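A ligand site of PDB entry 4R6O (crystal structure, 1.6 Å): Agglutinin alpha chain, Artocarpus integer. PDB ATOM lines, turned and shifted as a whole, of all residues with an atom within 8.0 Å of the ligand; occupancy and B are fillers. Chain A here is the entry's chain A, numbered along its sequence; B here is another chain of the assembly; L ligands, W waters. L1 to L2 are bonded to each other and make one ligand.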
ATOM      1  N   GLY A   1     -29.813 -17.964  18.263  1.00  0.00           N
ATOM      2  CA  GLY A   1     -31.203 -17.438  18.543  1.00  0.00           C
ATOM      3  C   GLY A   1     -32.273 -18.178  17.738  1.00  0.00           C
ATOM      4  O   GLY A   1     -32.003 -19.237  17.139  1.00  0.00           O
ATOM      5  N   LYS A   2     -33.486 -17.627  17.728  1.00  0.00           N
ATOM      6  CA  LYS A   2     -34.582 -18.256  16.992  1.00  0.00           C
ATOM      7  C   LYS A   2     -34.692 -17.769  15.522  1.00  0.00           C
ATOM      8  O   LYS A   2     -34.935 -16.571  15.328  1.00  0.00           O
ATOM      9  CB  LYS A   2     -35.891 -17.906  17.642  1.00  0.00           C
ATOM     10  CG  LYS A   2     -37.009 -18.768  17.089  1.00  0.00           C
ATOM     11  CD  LYS A   2     -38.328 -18.165  17.517  1.00  0.00           C
ATOM     12  CE  LYS A   2     -39.455 -19.177  17.344  1.00  0.00           C
ATOM     13  NZ  LYS A   2     -40.688 -18.586  17.958  1.00  0.00           N
ATOM     14  N   ALA A  24     -27.416  -3.626  20.654  1.00  0.00           N
ATOM     15  CA  ALA A  24     -27.746  -3.957  19.258  1.00  0.00           C
ATOM     16  C   ALA A  24     -29.283  -3.787  18.959  1.00  0.00           C
ATOM     17  O   ALA A  24     -30.041  -3.136  19.739  1.00  0.00           O
ATOM     18  CB  ALA A  24     -27.244  -5.325  18.896  1.00  0.00           C
ATOM     19  N   ILE A  25     -29.716  -4.320  17.806  1.00  0.00           N
ATOM     20  CA  ILE A  25     -31.157  -4.357  17.443  1.00  0.00           C
ATOM     21  C   ILE A  25     -31.720  -5.564  18.230  1.00  0.00           C
ATOM     22  O   ILE A  25     -31.032  -6.561  18.367  1.00  0.00           O
ATOM     23  CB  ILE A  25     -31.274  -4.647  15.944  1.00  0.00           C
ATOM     24  CG1 ILE A  25     -30.687  -3.441  15.138  1.00  0.00           C
ATOM     25  CG2 ILE A  25     -32.708  -5.085  15.498  1.00  0.00           C
ATOM     26  CD1 ILE A  25     -31.304  -2.101  15.427  1.00  0.00           C
ATOM     27  N   SER A  46     -36.989 -10.299  20.778  1.00  0.00           N
ATOM     28  CA  SER A  46     -35.767 -10.602  21.528  1.00  0.00           C
ATOM     29  C   SER A  46     -36.140 -11.499  22.717  1.00  0.00           C
ATOM     30  O   SER A  46     -37.205 -11.416  23.227  1.00  0.00           O
ATOM     31  CB  SER A  46     -35.191  -9.313  22.058  1.00  0.00           C
ATOM     32  OG  SER A  46     -34.079  -9.583  22.929  1.00  0.00           O
ATOM     33  N   PHE A  47     -35.195 -12.319  23.115  1.00  0.00           N
ATOM     34  CA  PHE A  47     -35.257 -13.098  24.383  1.00  0.00           C
ATOM     35  C   PHE A  47     -35.212 -12.204  25.651  1.00  0.00           C
ATOM     36  O   PHE A  47     -35.512 -12.700  26.778  1.00  0.00           O
ATOM     37  CB  PHE A  47     -34.061 -14.048  24.454  1.00  0.00           C
ATOM     38  CG  PHE A  47     -34.018 -15.167  23.421  1.00  0.00           C
ATOM     39  CD1 PHE A  47     -35.033 -15.406  22.463  1.00  0.00           C
ATOM     40  CD2 PHE A  47     -32.884 -16.012  23.406  1.00  0.00           C
ATOM     41  CE1 PHE A  47     -34.911 -16.480  21.550  1.00  0.00           C
ATOM     42  CE2 PHE A  47     -32.764 -17.082  22.517  1.00  0.00           C
ATOM     43  CZ  PHE A  47     -33.787 -17.316  21.571  1.00  0.00           C
ATOM     44  N   ILE A  48     -34.842 -10.936  25.536  1.00  0.00           N
ATOM     45  CA  ILE A  48     -34.751 -10.001  26.628  1.00  0.00           C
ATOM     46  C   ILE A  48     -35.579  -8.766  26.397  1.00  0.00           C
ATOM     47  O   ILE A  48     -36.080  -8.554  25.239  1.00  0.00           O
ATOM     48  CB  ILE A  48     -33.255  -9.656  26.966  1.00  0.00           C
ATOM     49  CG1 ILE A  48     -32.564  -9.016  25.735  1.00  0.00           C
ATOM     50  CG2 ILE A  48     -32.445 -10.914  27.321  1.00  0.00           C
ATOM     51  CD1 ILE A  48     -31.171  -8.474  26.093  1.00  0.00           C
ATOM     52  N   VAL A  75     -21.488  -8.293  20.714  1.00  0.00           N
ATOM     53  CA  VAL A  75     -22.214  -7.906  21.931  1.00  0.00           C
ATOM     54  C   VAL A  75     -22.249  -9.176  22.764  1.00  0.00           C
ATOM     55  O   VAL A  75     -22.590 -10.239  22.272  1.00  0.00           O
ATOM     56  CB  VAL A  75     -23.655  -7.386  21.698  1.00  0.00           C
ATOM     57  CG1 VAL A  75     -24.280  -6.957  23.033  1.00  0.00           C
ATOM     58  CG2 VAL A  75     -23.658  -6.208  20.709  1.00  0.00           C
ATOM     59  N   SER A  76     -21.748  -9.065  24.007  1.00  0.00           N
ATOM     60  CA  SER A  76     -21.571 -10.224  24.894  1.00  0.00           C
ATOM     61  C   SER A  76     -20.899 -11.398  24.210  1.00  0.00           C
ATOM     62  O   SER A  76     -21.174 -12.543  24.549  1.00  0.00           O
ATOM     63  CB  SER A  76     -22.909 -10.637  25.546  1.00  0.00           C
ATOM     64  OG  SER A  76     -23.628  -9.484  25.940  1.00  0.00           O
ATOM     65  N   GLY A  77     -19.991 -11.119  23.283  1.00  0.00           N
ATOM     66  CA  GLY A  77     -19.286 -12.239  22.625  1.00  0.00           C
ATOM     67  C   GLY A  77     -19.960 -12.834  21.379  1.00  0.00           C
ATOM     68  O   GLY A  77     -19.452 -13.778  20.768  1.00  0.00           O
ATOM     69  N   TYR A  78     -21.109 -12.262  20.998  1.00  0.00           N
ATOM     70  CA  TYR A  78     -21.875 -12.763  19.866  1.00  0.00           C
ATOM     71  C   TYR A  78     -21.793 -11.722  18.750  1.00  0.00           C
ATOM     72  O   TYR A  78     -21.877 -10.525  19.035  1.00  0.00           O
ATOM     73  CB  TYR A  78     -23.355 -12.948  20.240  1.00  0.00           C
ATOM     74  CG  TYR A  78     -23.549 -14.115  21.194  1.00  0.00           C
ATOM     75  CD1 TYR A  78     -23.716 -15.420  20.695  1.00  0.00           C
ATOM     76  CD2 TYR A  78     -23.528 -13.930  22.579  1.00  0.00           C
ATOM     77  CE1 TYR A  78     -23.878 -16.497  21.543  1.00  0.00           C
ATOM     78  CE2 TYR A  78     -23.696 -15.003  23.438  1.00  0.00           C
ATOM     79  CZ  TYR A  78     -23.848 -16.281  22.910  1.00  0.00           C
ATOM     80  OH  TYR A  78     -23.997 -17.343  23.768  1.00  0.00           O
ATOM     81  N   VAL A  79     -21.596 -12.216  17.523  1.00  0.00           N
ATOM     82  CA  VAL A  79     -21.712 -11.345  16.306  1.00  0.00           C
ATOM     83  C   VAL A  79     -23.185 -11.110  16.057  1.00  0.00           C
ATOM     84  O   VAL A  79     -23.922 -12.072  15.857  1.00  0.00           O
ATOM     85  CB  VAL A  79     -21.070 -11.944  15.044  1.00  0.00           C
ATOM     86  CG1 VAL A  79     -21.315 -11.015  13.818  1.00  0.00           C
ATOM     87  CG2 VAL A  79     -19.586 -12.154  15.281  1.00  0.00           C
ATOM     88  N   VAL A  80     -23.587  -9.854  16.138  1.00  0.00           N
ATOM     89  CA  VAL A  80     -25.022  -9.439  16.016  1.00  0.00           C
ATOM     90  C   VAL A  80     -25.147  -8.286  15.067  1.00  0.00           C
ATOM     91  O   VAL A  80     -24.135  -7.666  14.714  1.00  0.00           O
ATOM     92  CB  VAL A  80     -25.686  -9.126  17.358  1.00  0.00           C
ATOM     93  CG1 VAL A  80     -25.638 -10.396  18.200  1.00  0.00           C
ATOM     94  CG2 VAL A  80     -25.018  -7.966  18.100  1.00  0.00           C
ATOM     95  N   VAL A  81     -26.373  -7.993  14.676  1.00  0.00           N
ATOM     96  CA  VAL A  81     -26.649  -6.761  13.953  1.00  0.00           C
ATOM     97  C   VAL A  81     -26.736  -5.620  14.975  1.00  0.00           C
ATOM     98  O   VAL A  81     -27.775  -5.323  15.625  1.00  0.00           O
ATOM     99  CB  VAL A  81     -27.888  -6.893  12.974  1.00  0.00           C
ATOM    100  CG1 VAL A  81     -28.106  -5.582  12.219  1.00  0.00           C
ATOM    101  CG2 VAL A  81     -27.680  -8.113  12.082  1.00  0.00           C
ATOM    102  N   SER A 119     -32.559 -14.319  12.226  1.00  0.00           N
ATOM    103  CA  SER A 119     -32.613 -15.006  13.532  1.00  0.00           C
ATOM    104  C   SER A 119     -32.477 -13.965  14.652  1.00  0.00           C
ATOM    105  O   SER A 119     -31.757 -12.964  14.512  1.00  0.00           O
ATOM    106  CB  SER A 119     -31.457 -16.001  13.542  1.00  0.00           C
ATOM    107  OG  SER A 119     -31.285 -16.597  14.848  1.00  0.00           O
ATOM    108  N   ILE A 120     -33.148 -14.195  15.783  1.00  0.00           N
ATOM    109  CA  ILE A 120     -33.085 -13.262  16.911  1.00  0.00           C
ATOM    110  C   ILE A 120     -32.927 -14.103  18.187  1.00  0.00           C
ATOM    111  O   ILE A 120     -33.696 -15.027  18.406  1.00  0.00           O
ATOM    112  CB  ILE A 120     -34.331 -12.356  16.979  1.00  0.00           C
ATOM    113  CG1 ILE A 120     -34.522 -11.511  15.680  1.00  0.00           C
ATOM    114  CG2 ILE A 120     -34.272 -11.368  18.126  1.00  0.00           C
ATOM    115  CD1 ILE A 120     -35.652 -10.509  15.782  1.00  0.00           C
ATOM    116  N   GLY A 121     -31.889 -13.775  18.942  1.00  0.00           N
ATOM    117  CA  GLY A 121     -31.655 -14.346  20.322  1.00  0.00           C
ATOM    118  C   GLY A 121     -31.819 -13.174  21.264  1.00  0.00           C
ATOM    119  O   GLY A 121     -32.884 -12.516  21.313  1.00  0.00           O
ATOM    120  N   TYR A 122     -30.757 -12.805  22.017  1.00  0.00           N
ATOM    121  CA  TYR A 122     -30.911 -11.575  22.761  1.00  0.00           C
ATOM    122  C   TYR A 122     -30.965 -10.369  21.773  1.00  0.00           C
ATOM    123  O   TYR A 122     -31.655  -9.375  22.002  1.00  0.00           O
ATOM    124  CB  TYR A 122     -29.779 -11.313  23.768  1.00  0.00           C
ATOM    125  CG  TYR A 122     -29.807 -12.159  25.050  1.00  0.00           C
ATOM    126  CD1 TYR A 122     -30.290 -13.444  25.053  1.00  0.00           C
ATOM    127  CD2 TYR A 122     -29.244 -11.640  26.213  1.00  0.00           C
ATOM    128  CE1 TYR A 122     -30.293 -14.207  26.210  1.00  0.00           C
ATOM    129  CE2 TYR A 122     -29.217 -12.421  27.379  1.00  0.00           C
ATOM    130  CZ  TYR A 122     -29.753 -13.648  27.368  1.00  0.00           C
ATOM    131  OH  TYR A 122     -29.678 -14.352  28.576  1.00  0.00           O
ATOM    132  N   TRP A 123     -30.210 -10.520  20.689  1.00  0.00           N
ATOM    133  CA  TRP A 123     -30.236  -9.434  19.654  1.00  0.00           C
ATOM    134  C   TRP A 123     -30.454 -10.064  18.332  1.00  0.00           C
ATOM    135  O   TRP A 123     -30.373 -11.246  18.173  1.00  0.00           O
ATOM    136  CB  TRP A 123     -28.992  -8.534  19.708  1.00  0.00           C
ATOM    137  CG  TRP A 123     -28.797  -7.975  21.117  1.00  0.00           C
ATOM    138  CD1 TRP A 123     -29.426  -6.894  21.724  1.00  0.00           C
ATOM    139  CD2 TRP A 123     -27.951  -8.583  22.147  1.00  0.00           C
ATOM    140  NE1 TRP A 123     -29.014  -6.781  23.070  1.00  0.00           N
ATOM    141  CE2 TRP A 123     -28.138  -7.775  23.355  1.00  0.00           C
ATOM    142  CE3 TRP A 123     -27.114  -9.702  22.183  1.00  0.00           C
ATOM    143  CZ2 TRP A 123     -27.475  -8.081  24.577  1.00  0.00           C
ATOM    144  CZ3 TRP A 123     -26.429  -9.984  23.418  1.00  0.00           C
ATOM    145  CH2 TRP A 123     -26.653  -9.196  24.557  1.00  0.00           C
ATOM    146  N   LEU A 124     -30.739  -9.229  17.316  1.00  0.00           N
ATOM    147  CA  LEU A 124     -30.812  -9.719  15.939  1.00  0.00           C
ATOM    148  C   LEU A 124     -29.454 -10.369  15.476  1.00  0.00           C
ATOM    149  O   LEU A 124     -28.433  -9.685  15.424  1.00  0.00           O
ATOM    150  CB  LEU A 124     -31.223  -8.536  15.043  1.00  0.00           C
ATOM    151  CG  LEU A 124     -31.277  -8.849  13.521  1.00  0.00           C
ATOM    152  CD1 LEU A 124     -32.320  -9.890  13.147  1.00  0.00           C
ATOM    153  CD2 LEU A 124     -31.536  -7.550  12.745  1.00  0.00           C
ATOM    154  N   ASP A 125     -29.443 -11.667  15.277  1.00  0.00           N
ATOM    155  CA  ASP A 125     -28.197 -12.413  14.988  1.00  0.00           C
ATOM    156  C   ASP A 125     -27.698 -12.154  13.563  1.00  0.00           C
ATOM    157  O   ASP A 125     -26.531 -11.795  13.351  1.00  0.00           O
ATOM    158  CB  ASP A 125     -28.367 -13.891  15.170  1.00  0.00           C
ATOM    159  CG  ASP A 125     -28.854 -14.246  16.572  1.00  0.00           C
ATOM    160  OD1 ASP A 125     -28.250 -13.706  17.538  1.00  0.00           O
ATOM    161  OD2 ASP A 125     -29.858 -14.996  16.653  1.00  0.00           O
ATOM    162  N   TYR A 126     -28.636 -12.255  12.596  1.00  0.00           N
ATOM    163  CA  TYR A 126     -28.283 -12.058  11.166  1.00  0.00           C
ATOM    164  C   TYR A 126     -29.609 -11.899  10.436  1.00  0.00           C
ATOM    165  O   TYR A 126     -30.683 -12.261  10.978  1.00  0.00           O
ATOM    166  CB  TYR A 126     -27.531 -13.229  10.586  1.00  0.00           C
ATOM    167  CG  TYR A 126     -28.229 -14.566  10.732  1.00  0.00           C
ATOM    168  CD1 TYR A 126     -29.247 -14.943   9.850  1.00  0.00           C
ATOM    169  CD2 TYR A 126     -27.840 -15.490  11.737  1.00  0.00           C
ATOM    170  CE1 TYR A 126     -29.884 -16.172   9.962  1.00  0.00           C
ATOM    171  CE2 TYR A 126     -28.476 -16.707  11.881  1.00  0.00           C
ATOM    172  CZ  TYR A 126     -29.489 -17.054  10.997  1.00  0.00           C
ATOM    173  OH  TYR A 126     -30.118 -18.272  11.083  1.00  0.00           O
ATOM    174  N   ALA B  16     -24.026 -12.812  12.195  1.00  0.00           N
ATOM    175  CA  ALA B  16     -23.349 -14.054  12.510  1.00  0.00           C
ATOM    176  C   ALA B  16     -23.426 -15.083  11.379  1.00  0.00           C
ATOM    177  O   ALA B  16     -24.443 -15.208  10.720  1.00  0.00           O
ATOM    178  CB  ALA B  16     -23.955 -14.640  13.782  1.00  0.00           C
HETATM  179  O1  LIG L   1     -24.972 -15.260  30.454  1.00  0.00           O
HETATM  180  C1  LIG L   1     -25.279 -14.713  29.395  1.00  0.00           C
HETATM  181  O2  LIG L   1     -25.731 -15.447  28.324  1.00  0.00           O
HETATM  182  C2  LIG L   1     -26.031 -14.821  27.147  1.00  0.00           C
HETATM  183  C3  LIG L   1     -26.440 -15.604  26.071  1.00  0.00           C
HETATM  184  C4  LIG L   1     -26.754 -14.964  24.869  1.00  0.00           C
HETATM  185  C5  LIG L   1     -26.632 -13.597  24.776  1.00  0.00           C
HETATM  186  C6  LIG L   1     -26.199 -12.811  25.857  1.00  0.00           C
HETATM  187  C7  LIG L   1     -25.901 -13.411  27.067  1.00  0.00           C
HETATM  188  C8  LIG L   1     -25.474 -12.650  28.173  1.00  0.00           C
HETATM  189  C9  LIG L   1     -25.371 -11.250  28.152  1.00  0.00           C
HETATM  190  C10 LIG L   1     -25.190 -13.320  29.341  1.00  0.00           C
HETATM  191  C1  LG2 L   2     -28.393 -15.541  23.052  1.00  0.00           C
HETATM  192  C2  LG2 L   2     -28.632 -16.752  22.215  1.00  0.00           C
HETATM  193  C3  LG2 L   2     -27.536 -16.977  21.106  1.00  0.00           C
HETATM  194  C4  LG2 L   2     -27.450 -15.681  20.250  1.00  0.00           C
HETATM  195  C5  LG2 L   2     -27.223 -14.510  21.239  1.00  0.00           C
HETATM  196  C6  LG2 L   2     -27.110 -13.147  20.552  1.00  0.00           C
HETATM  197  O1  LG2 L   2     -27.142 -15.771  23.853  1.00  0.00           O
HETATM  198  O2  LG2 L   2     -28.657 -17.871  23.070  1.00  0.00           O
HETATM  199  O3  LG2 L   2     -27.821 -18.161  20.282  1.00  0.00           O
HETATM  200  O4  LG2 L   2     -28.691 -15.525  19.559  1.00  0.00           O
HETATM  201  O5  LG2 L   2     -28.309 -14.406  22.210  1.00  0.00           O
HETATM  202  O6  LG2 L   2     -28.418 -12.652  20.227  1.00  0.00           O
HETATM  203  O   HOH W   1     -28.573 -20.322  21.863  1.00  0.00           O
HETATM  204  O   HOH W   2     -26.193 -18.599  24.333  1.00  0.00           O
HETATM  205  O   HOH W   3     -22.526  -9.479  28.593  1.00  0.00           O
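Water W2 bridges the side-chain hydroxyl (OH) of Tyr 78 (2.6 Å) and an oxygen (O2) of LG2 L2 (2.9 Å).
The backbone NH of Gly 1 lies close to the side-chain carboxylate of Asp 125 (3.4 Å).
OD2 of Asp 125 lies within hydrogen-bond range of N of Gly 121 (3.3 Å).
OD2 of Asp 125 lies within hydrogen-bond range of N of Ile 120 (3.5 Å).
The backbone carbonyl oxygen (O) of Ser 119 lies within hydrogen-bond range of the backbone NH (N) of Asp 125 (2.8 Å).
N of Ala 16 of chain B lies within hydrogen-bond range of O of Asp 125 (2.9 Å).
The backbone carbonyl oxygen (O) of Tyr 122 lies within hydrogen-bond range of the side-chain hydroxyl (OG) of Ser 46, 2.6 Å away.
N of Phe 47 sits at hydrogen-bond distance from O of Gly 121 (2.9 Å).
OD1 of Asp 125 sits at hydrogen-bond distance from O4 of LG2 L2 (2.8 Å).
N of Trp 123 sits at hydrogen-bond distance from O6 of LG2 L2 (2.8 Å).
The backbone carbonyl oxygen of Trp 123 lies within hydrogen-bond range of an oxygen (O6) of LG2 L2 (3.2 Å).
The backbone NH (N) of Gly 1 lies within hydrogen-bond range of an oxygen (O3) of LG2 L2 (2.8 Å).
The backbone NH (N) of Tyr 122 lies within hydrogen-bond range of an oxygen (O5) of LG2 L2, at 2.9 Å.
Residues that only touch the ligand: Ser 76, Tyr 78, Val 80 and Gly 121.
Hydrophobic or aromatic side chains within 4 Å of the ligand: Tyr 78, Val 80, Tyr 122 and Trp 123.
Eight residues have an atom within 4 Å of the ligand: Gly 1, Ser 76, Tyr 78, Val 80, Gly 121, Tyr 122, Trp 123 and Asp 125.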
